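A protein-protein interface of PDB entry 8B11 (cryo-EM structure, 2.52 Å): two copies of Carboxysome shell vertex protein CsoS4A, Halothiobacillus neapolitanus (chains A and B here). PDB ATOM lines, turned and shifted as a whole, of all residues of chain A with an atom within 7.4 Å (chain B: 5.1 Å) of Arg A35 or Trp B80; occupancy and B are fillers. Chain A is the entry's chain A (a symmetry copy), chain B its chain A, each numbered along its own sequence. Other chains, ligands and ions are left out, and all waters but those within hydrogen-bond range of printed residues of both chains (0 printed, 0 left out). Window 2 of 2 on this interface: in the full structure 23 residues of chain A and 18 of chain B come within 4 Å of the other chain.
No position is printed for both chains.
Of the 6 pairs that touch across the chains among the printed residues, none has its exchanged pair printed and touching as well.
Of chain B, only Trp B80 comes within 4 Å of Arg A35.
Trp B80 touches just one residue of chain A: Arg A35.
Of the printed residues of chain B, Leu A10 touches Ile B3 and Ile B77.
Printed residues of chain A within 4 Å of Lys B2: Gln A36.
Printed residues of chain B within 4 Å of Gln A36: Lys B2 (3.6 Å).
Of the printed residues of chain A, Ile B3 touches Leu A10 and Val A37.
Thr A9 touches none of the printed residues of chain B.
The nearest residue of chain B that does not touch Arg A35 is Lys B2 (4.7 Å).
O of Val A11 sits at hydrogen-bond distance from N of Asp B78 (3.2 Å).
NH2 of Arg A35 lies within salt-bridge range of OE1 of Glu A7 (2.8 Å).
The backbone carbonyl oxygen (O) of Val A27 lies within hydrogen-bond range of the backbone NH (N) of Gln A36 (2.9 Å).
The backbone carbonyl oxygen (O) of Trp B49 is in hydrogen-bond range of the backbone NH (N) of Ile B77, at 2.9 Å.
Leu A10 touches Ile B3 (CD1 to CD1, 3.4 Å).
Leu A10 touches Ile B77 (CD1 to CD1, 3.8 Å).
Trp B80 touches Arg A35 (CZ2 to NE, 3.6 Å).
NE2 of Gln A36 touches NZ of Lys B2, at 3.6 Å.
CG2 of Val A37 touches CG1 of Ile B3, 3.7 Å away.
Of the 18 printed residues of chain A, 5 touch a printed residue of chain B.
Printed residues of chain A that touch a printed residue of chain B: Leu A10, Val A11, Arg A35, Gln A36 and Val A37.
Hydrophobic or aromatic side chains of chain A within 4 Å of the printed part of chain B: Leu A10, Val A11 and Val A37.
Hydrophobic or aromatic side chains of chain B within 4 Å of the printed part of chain A: Ile B3, Ile B77 and Trp B80.
Among the printed residues, 6 pairs touch across the chains.
Among the printed residues, no Asp or Glu carboxylate lies within 4 Å of a Lys or Arg side-chain nitrogen of the other chain.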
ATOM      1  N   MET A   4     -13.039  28.976  13.150  1.00  0.00           N
ATOM      2  CA  MET A   4     -14.279  28.795  12.417  1.00  0.00           C
ATOM      3  C   MET A   4     -14.100  29.302  10.999  1.00  0.00           C
ATOM      4  O   MET A   4     -13.182  30.061  10.700  1.00  0.00           O
ATOM      5  CB  MET A   4     -15.431  29.543  13.097  1.00  0.00           C
ATOM      6  CG  MET A   4     -15.722  29.090  14.508  1.00  0.00           C
ATOM      7  SD  MET A   4     -16.789  27.651  14.607  1.00  0.00           S
ATOM      8  CE  MET A   4     -17.656  28.016  16.123  1.00  0.00           C
ATOM      9  N   GLU A   7     -19.627  31.079   6.969  1.00  0.00           N
ATOM     10  CA  GLU A   7     -20.504  30.658   5.883  1.00  0.00           C
ATOM     11  C   GLU A   7     -21.181  31.846   5.219  1.00  0.00           C
ATOM     12  O   GLU A   7     -20.980  32.104   4.028  1.00  0.00           O
ATOM     13  CB  GLU A   7     -21.570  29.681   6.378  1.00  0.00           C
ATOM     14  CG  GLU A   7     -21.924  28.627   5.355  1.00  0.00           C
ATOM     15  CD  GLU A   7     -23.322  28.074   5.544  1.00  0.00           C
ATOM     16  OE1 GLU A   7     -23.681  27.089   4.868  1.00  0.00           O
ATOM     17  OE2 GLU A   7     -24.080  28.633   6.356  1.00  0.00           O
ATOM     18  N   LYS A   8     -21.995  32.578   5.970  1.00  0.00           N
ATOM     19  CA  LYS A   8     -22.761  33.659   5.355  1.00  0.00           C
ATOM     20  C   LYS A   8     -23.155  34.663   6.424  1.00  0.00           C
ATOM     21  O   LYS A   8     -22.641  34.641   7.544  1.00  0.00           O
ATOM     22  CB  LYS A   8     -24.004  33.131   4.632  1.00  0.00           C
ATOM     23  CG  LYS A   8     -24.643  31.921   5.267  1.00  0.00           C
ATOM     24  CD  LYS A   8     -25.931  31.577   4.557  1.00  0.00           C
ATOM     25  CE  LYS A   8     -26.505  30.261   5.033  1.00  0.00           C
ATOM     26  NZ  LYS A   8     -26.123  29.151   4.116  1.00  0.00           N
ATOM     27  N   THR A   9     -24.076  35.547   6.071  1.00  0.00           N
ATOM     28  CA  THR A   9     -24.643  36.511   6.995  1.00  0.00           C
ATOM     29  C   THR A   9     -26.018  36.035   7.437  1.00  0.00           C
ATOM     30  O   THR A   9     -26.669  35.243   6.754  1.00  0.00           O
ATOM     31  CB  THR A   9     -24.755  37.892   6.347  1.00  0.00           C
ATOM     32  OG1 THR A   9     -25.843  37.893   5.416  1.00  0.00           O
ATOM     33  CG2 THR A   9     -23.478  38.231   5.605  1.00  0.00           C
ATOM     34  N   LEU A  10     -26.456  36.522   8.592  1.00  0.00           N
ATOM     35  CA  LEU A  10     -27.780  36.210   9.101  1.00  0.00           C
ATOM     36  C   LEU A  10     -28.464  37.501   9.517  1.00  0.00           C
ATOM     37  O   LEU A  10     -27.848  38.349  10.168  1.00  0.00           O
ATOM     38  CB  LEU A  10     -27.707  35.232  10.276  1.00  0.00           C
ATOM     39  CG  LEU A  10     -29.048  34.702  10.774  1.00  0.00           C
ATOM     40  CD1 LEU A  10     -28.978  33.210  11.019  1.00  0.00           C
ATOM     41  CD2 LEU A  10     -29.455  35.432  12.039  1.00  0.00           C
ATOM     42  N   VAL A  11     -29.729  37.643   9.142  1.00  0.00           N
ATOM     43  CA  VAL A  11     -30.528  38.814   9.473  1.00  0.00           C
ATOM     44  C   VAL A  11     -31.723  38.354  10.292  1.00  0.00           C
ATOM     45  O   VAL A  11     -32.463  37.455   9.873  1.00  0.00           O
ATOM     46  CB  VAL A  11     -30.984  39.569   8.215  1.00  0.00           C
ATOM     47  CG1 VAL A  11     -32.054  40.595   8.564  1.00  0.00           C
ATOM     48  CG2 VAL A  11     -29.797  40.231   7.539  1.00  0.00           C
ATOM     49  N   VAL A  26     -23.267  33.500  10.075  1.00  0.00           N
ATOM     50  CA  VAL A  26     -23.350  32.055  10.213  1.00  0.00           C
ATOM     51  C   VAL A  26     -21.973  31.486   9.905  1.00  0.00           C
ATOM     52  O   VAL A  26     -21.433  31.708   8.814  1.00  0.00           O
ATOM     53  CB  VAL A  26     -24.411  31.458   9.280  1.00  0.00           C
ATOM     54  CG1 VAL A  26     -24.207  29.966   9.160  1.00  0.00           C
ATOM     55  CG2 VAL A  26     -25.800  31.776   9.783  1.00  0.00           C
ATOM     56  N   VAL A  27     -21.418  30.747  10.863  1.00  0.00           N
ATOM     57  CA  VAL A  27     -20.093  30.154  10.779  1.00  0.00           C
ATOM     58  C   VAL A  27     -20.186  28.682  11.143  1.00  0.00           C
ATOM     59  O   VAL A  27     -21.075  28.260  11.887  1.00  0.00           O
ATOM     60  CB  VAL A  27     -19.078  30.861  11.708  1.00  0.00           C
ATOM     61  CG1 VAL A  27     -18.921  32.315  11.329  1.00  0.00           C
ATOM     62  CG2 VAL A  27     -19.513  30.734  13.160  1.00  0.00           C
ATOM     63  N   TRP A  28     -19.271  27.895  10.601  1.00  0.00           N
ATOM     64  CA  TRP A  28     -19.050  26.524  11.027  1.00  0.00           C
ATOM     65  C   TRP A  28     -17.572  26.318  11.324  1.00  0.00           C
ATOM     66  O   TRP A  28     -16.718  27.109  10.923  1.00  0.00           O
ATOM     67  CB  TRP A  28     -19.514  25.507   9.980  1.00  0.00           C
ATOM     68  CG  TRP A  28     -19.174  25.849   8.565  1.00  0.00           C
ATOM     69  CD1 TRP A  28     -17.987  26.329   8.097  1.00  0.00           C
ATOM     70  CD2 TRP A  28     -19.979  25.593   7.412  1.00  0.00           C
ATOM     71  NE1 TRP A  28     -18.038  26.469   6.735  1.00  0.00           N
ATOM     72  CE2 TRP A  28     -19.248  26.011   6.289  1.00  0.00           C
ATOM     73  CE3 TRP A  28     -21.262  25.074   7.226  1.00  0.00           C
ATOM     74  CZ2 TRP A  28     -19.753  25.928   4.997  1.00  0.00           C
ATOM     75  CZ3 TRP A  28     -21.764  24.994   5.944  1.00  0.00           C
ATOM     76  CH2 TRP A  28     -21.011  25.419   4.844  1.00  0.00           C
ATOM     77  N   GLU A  29     -17.273  25.232  12.037  1.00  0.00           N
ATOM     78  CA  GLU A  29     -15.880  24.854  12.227  1.00  0.00           C
ATOM     79  C   GLU A  29     -15.263  24.415  10.908  1.00  0.00           C
ATOM     80  O   GLU A  29     -14.148  24.819  10.564  1.00  0.00           O
ATOM     81  CB  GLU A  29     -15.769  23.740  13.269  1.00  0.00           C
ATOM     82  CG  GLU A  29     -16.101  24.184  14.678  1.00  0.00           C
ATOM     83  CD  GLU A  29     -15.894  23.091  15.706  1.00  0.00           C
ATOM     84  OE1 GLU A  29     -15.583  21.949  15.312  1.00  0.00           O
ATOM     85  OE2 GLU A  29     -16.056  23.370  16.911  1.00  0.00           O
ATOM     86  N   LYS A  30     -15.984  23.591  10.160  1.00  0.00           N
ATOM     87  CA  LYS A  30     -15.597  23.106   8.849  1.00  0.00           C
ATOM     88  C   LYS A  30     -16.855  22.915   8.017  1.00  0.00           C
ATOM     89  O   LYS A  30     -17.949  22.766   8.575  1.00  0.00           O
ATOM     90  CB  LYS A  30     -14.809  21.793   8.972  1.00  0.00           C
ATOM     91  CG  LYS A  30     -15.657  20.561   9.204  1.00  0.00           C
ATOM     92  CD  LYS A  30     -14.908  19.599  10.109  1.00  0.00           C
ATOM     93  CE  LYS A  30     -14.865  18.190   9.561  1.00  0.00           C
ATOM     94  NZ  LYS A  30     -14.200  17.277  10.534  1.00  0.00           N
ATOM     95  N   GLY A  32     -19.926  21.558   6.492  1.00  0.00           N
ATOM     96  CA  GLY A  32     -20.723  20.416   6.877  1.00  0.00           C
ATOM     97  C   GLY A  32     -20.929  20.265   8.369  1.00  0.00           C
ATOM     98  O   GLY A  32     -21.831  19.525   8.781  1.00  0.00           O
ATOM     99  N   ALA A  33     -20.128  20.945   9.186  1.00  0.00           N
ATOM    100  CA  ALA A  33     -20.283  20.900  10.626  1.00  0.00           C
ATOM    101  C   ALA A  33     -21.534  21.671  11.043  1.00  0.00           C
ATOM    102  O   ALA A  33     -22.080  22.448  10.258  1.00  0.00           O
ATOM    103  CB  ALA A  33     -19.043  21.481  11.303  1.00  0.00           C
ATOM    104  N   PRO A  34     -22.029  21.449  12.264  1.00  0.00           N
ATOM    105  CA  PRO A  34     -23.188  22.220  12.728  1.00  0.00           C
ATOM    106  C   PRO A  34     -22.919  23.717  12.684  1.00  0.00           C
ATOM    107  O   PRO A  34     -21.847  24.189  13.067  1.00  0.00           O
ATOM    108  CB  PRO A  34     -23.383  21.731  14.167  1.00  0.00           C
ATOM    109  CG  PRO A  34     -22.805  20.371  14.176  1.00  0.00           C
ATOM    110  CD  PRO A  34     -21.645  20.404  13.231  1.00  0.00           C
ATOM    111  N   ARG A  35     -23.914  24.464  12.219  1.00  0.00           N
ATOM    112  CA  ARG A  35     -23.785  25.906  12.106  1.00  0.00           C
ATOM    113  C   ARG A  35     -23.957  26.571  13.463  1.00  0.00           C
ATOM    114  O   ARG A  35     -24.643  26.061  14.350  1.00  0.00           O
ATOM    115  CB  ARG A  35     -24.813  26.477  11.133  1.00  0.00           C
ATOM    116  CG  ARG A  35     -24.805  25.864   9.751  1.00  0.00           C
ATOM    117  CD  ARG A  35     -26.219  25.813   9.220  1.00  0.00           C
ATOM    118  NE  ARG A  35     -26.318  26.222   7.825  1.00  0.00           N
ATOM    119  CZ  ARG A  35     -26.042  25.439   6.794  1.00  0.00           C
ATOM    120  NH1 ARG A  35     -25.660  24.185   6.961  1.00  0.00           N
ATOM    121  NH2 ARG A  35     -26.171  25.920   5.563  1.00  0.00           N
ATOM    122  N   GLN A  36     -23.317  27.723  13.613  1.00  0.00           N
ATOM    123  CA  GLN A  36     -23.514  28.618  14.740  1.00  0.00           C
ATOM    124  C   GLN A  36     -23.591  30.042  14.216  1.00  0.00           C
ATOM    125  O   GLN A  36     -23.245  30.324  13.068  1.00  0.00           O
ATOM    126  CB  GLN A  36     -22.391  28.501  15.771  1.00  0.00           C
ATOM    127  CG  GLN A  36     -22.536  27.350  16.725  1.00  0.00           C
ATOM    128  CD  GLN A  36     -21.218  26.689  17.008  1.00  0.00           C
ATOM    129  OE1 GLN A  36     -20.521  26.257  16.093  1.00  0.00           O
ATOM    130  NE2 GLN A  36     -20.847  26.633  18.278  1.00  0.00           N
ATOM    131  N   VAL A  37     -24.055  30.947  15.067  1.00  0.00           N
ATOM    132  CA  VAL A  37     -24.142  32.360  14.736  1.00  0.00           C
ATOM    133  C   VAL A  37     -23.211  33.127  15.662  1.00  0.00           C
ATOM    134  O   VAL A  37     -23.280  32.977  16.886  1.00  0.00           O
ATOM    135  CB  VAL A  37     -25.585  32.882  14.838  1.00  0.00           C
ATOM    136  CG1 VAL A  37     -25.640  34.357  14.489  1.00  0.00           C
ATOM    137  CG2 VAL A  37     -26.484  32.082  13.922  1.00  0.00           C
ATOM    138  N   LEU A  71     -21.117  34.050  21.351  1.00  0.00           N
ATOM    139  CA  LEU A  71     -20.117  33.724  20.336  1.00  0.00           C
ATOM    140  C   LEU A  71     -19.816  34.990  19.554  1.00  0.00           C
ATOM    141  O   LEU A  71     -20.716  35.556  18.927  1.00  0.00           O
ATOM    142  CB  LEU A  71     -20.604  32.621  19.402  1.00  0.00           C
ATOM    143  CG  LEU A  71     -19.503  32.020  18.528  1.00  0.00           C
ATOM    144  CD1 LEU A  71     -18.496  31.284  19.392  1.00  0.00           C
ATOM    145  CD2 LEU A  71     -20.076  31.102  17.472  1.00  0.00           C
ATOM    146  N   LYS B   2     -26.864  29.780  18.681  1.00  0.00           N
ATOM    147  CA  LYS B   2     -27.255  28.604  17.924  1.00  0.00           C
ATOM    148  C   LYS B   2     -28.558  28.879  17.186  1.00  0.00           C
ATOM    149  O   LYS B   2     -29.362  29.720  17.597  1.00  0.00           O
ATOM    150  CB  LYS B   2     -27.421  27.389  18.838  1.00  0.00           C
ATOM    151  CG  LYS B   2     -26.312  26.362  18.723  1.00  0.00           C
ATOM    152  CD  LYS B   2     -26.113  25.626  20.038  1.00  0.00           C
ATOM    153  CE  LYS B   2     -24.852  24.774  20.025  1.00  0.00           C
ATOM    154  NZ  LYS B   2     -23.630  25.562  20.344  1.00  0.00           N
ATOM    155  N   ILE B   3     -28.753  28.163  16.087  1.00  0.00           N
ATOM    156  CA  ILE B   3     -29.946  28.300  15.265  1.00  0.00           C
ATOM    157  C   ILE B   3     -30.848  27.119  15.586  1.00  0.00           C
ATOM    158  O   ILE B   3     -30.458  25.960  15.403  1.00  0.00           O
ATOM    159  CB  ILE B   3     -29.592  28.350  13.773  1.00  0.00           C
ATOM    160  CG1 ILE B   3     -29.328  29.791  13.352  1.00  0.00           C
ATOM    161  CG2 ILE B   3     -30.738  27.818  12.938  1.00  0.00           C
ATOM    162  CD1 ILE B   3     -28.884  29.929  11.919  1.00  0.00           C
ATOM    163  N   TRP B  49     -37.777  29.368  13.001  1.00  0.00           N
ATOM    164  CA  TRP B  49     -36.337  29.258  13.171  1.00  0.00           C
ATOM    165  C   TRP B  49     -35.876  30.470  13.966  1.00  0.00           C
ATOM    166  O   TRP B  49     -36.146  31.611  13.581  1.00  0.00           O
ATOM    167  CB  TRP B  49     -35.629  29.179  11.821  1.00  0.00           C
ATOM    168  CG  TRP B  49     -35.822  27.860  11.156  1.00  0.00           C
ATOM    169  CD1 TRP B  49     -36.680  27.577  10.141  1.00  0.00           C
ATOM    170  CD2 TRP B  49     -35.158  26.635  11.473  1.00  0.00           C
ATOM    171  NE1 TRP B  49     -36.588  26.255   9.796  1.00  0.00           N
ATOM    172  CE2 TRP B  49     -35.658  25.652  10.600  1.00  0.00           C
ATOM    173  CE3 TRP B  49     -34.184  26.273  12.406  1.00  0.00           C
ATOM    174  CZ2 TRP B  49     -35.219  24.335  10.631  1.00  0.00           C
ATOM    175  CZ3 TRP B  49     -33.748  24.967  12.435  1.00  0.00           C
ATOM    176  CH2 TRP B  49     -34.264  24.014  11.554  1.00  0.00           C
ATOM    177  N   ILE B  77     -35.302  34.303  12.798  1.00  0.00           N
ATOM    178  CA  ILE B  77     -34.559  34.436  11.554  1.00  0.00           C
ATOM    179  C   ILE B  77     -35.521  34.781  10.426  1.00  0.00           C
ATOM    180  O   ILE B  77     -36.533  34.100  10.220  1.00  0.00           O
ATOM    181  CB  ILE B  77     -33.779  33.149  11.258  1.00  0.00           C
ATOM    182  CG1 ILE B  77     -32.902  32.790  12.454  1.00  0.00           C
ATOM    183  CG2 ILE B  77     -32.936  33.309  10.008  1.00  0.00           C
ATOM    184  CD1 ILE B  77     -32.167  31.519  12.280  1.00  0.00           C
ATOM    185  N   ASP B  78     -35.208  35.850   9.692  1.00  0.00           N
ATOM    186  CA  ASP B  78     -36.084  36.290   8.612  1.00  0.00           C
ATOM    187  C   ASP B  78     -36.242  35.213   7.549  1.00  0.00           C
ATOM    188  O   ASP B  78     -37.354  34.958   7.074  1.00  0.00           O
ATOM    189  CB  ASP B  78     -35.545  37.578   7.993  1.00  0.00           C
ATOM    190  CG  ASP B  78     -35.720  38.781   8.901  1.00  0.00           C
ATOM    191  OD1 ASP B  78     -36.296  38.623   9.996  1.00  0.00           O
ATOM    192  OD2 ASP B  78     -35.284  39.882   8.521  1.00  0.00           O
ATOM    193  N   GLN B  79     -35.147  34.563   7.168  1.00  0.00           N
ATOM    194  CA  GLN B  79     -35.164  33.596   6.077  1.00  0.00           C
ATOM    195  C   GLN B  79     -34.298  32.407   6.467  1.00  0.00           C
ATOM    196  O   GLN B  79     -33.068  32.510   6.471  1.00  0.00           O
ATOM    197  CB  GLN B  79     -34.670  34.232   4.779  1.00  0.00           C
ATOM    198  CG  GLN B  79     -35.781  34.609   3.815  1.00  0.00           C
ATOM    199  CD  GLN B  79     -36.292  36.020   4.041  1.00  0.00           C
ATOM    200  OE1 GLN B  79     -35.609  36.999   3.736  1.00  0.00           O
ATOM    201  NE2 GLN B  79     -37.502  36.132   4.578  1.00  0.00           N
ATOM    202  N   TRP B  80     -34.935  31.287   6.791  1.00  0.00           N
ATOM    203  CA  TRP B  80     -34.221  30.059   7.104  1.00  0.00           C
ATOM    204  C   TRP B  80     -35.116  28.879   6.762  1.00  0.00           C
ATOM    205  O   TRP B  80     -36.339  29.009   6.679  1.00  0.00           O
ATOM    206  CB  TRP B  80     -33.803  30.005   8.576  1.00  0.00           C
ATOM    207  CG  TRP B  80     -32.698  29.041   8.836  1.00  0.00           C
ATOM    208  CD1 TRP B  80     -32.816  27.763   9.291  1.00  0.00           C
ATOM    209  CD2 TRP B  80     -31.300  29.273   8.648  1.00  0.00           C
ATOM    210  NE1 TRP B  80     -31.577  27.184   9.401  1.00  0.00           N
ATOM    211  CE2 TRP B  80     -30.629  28.090   9.011  1.00  0.00           C
ATOM    212  CE3 TRP B  80     -30.550  30.368   8.210  1.00  0.00           C
ATOM    213  CZ2 TRP B  80     -29.246  27.970   8.952  1.00  0.00           C
ATOM    214  CZ3 TRP B  80     -29.177  30.246   8.149  1.00  0.00           C
ATOM    215  CH2 TRP B  80     -28.538  29.057   8.519  1.00  0.00           C
ATOM    216  N   ASN B  81     -34.490  27.725   6.574  1.00  0.00           N
ATOM    217  CA  ASN B  81     -35.224  26.502   6.273  1.00  0.00           C
ATOM    218  C   ASN B  81     -34.437  25.274   6.722  1.00  0.00           C
ATOM    219  O   ASN B  81     -33.208  25.278   6.715  1.00  0.00           O
ATOM    220  CB  ASN B  81     -35.529  26.420   4.778  1.00  0.00           C
ATOM    221  CG  ASN B  81     -34.351  26.833   3.928  1.00  0.00           C
ATOM    222  OD1 ASN B  81     -33.308  27.224   4.447  1.00  0.00           O
ATOM    223  ND2 ASN B  81     -34.512  26.756   2.615  1.00  0.00           N
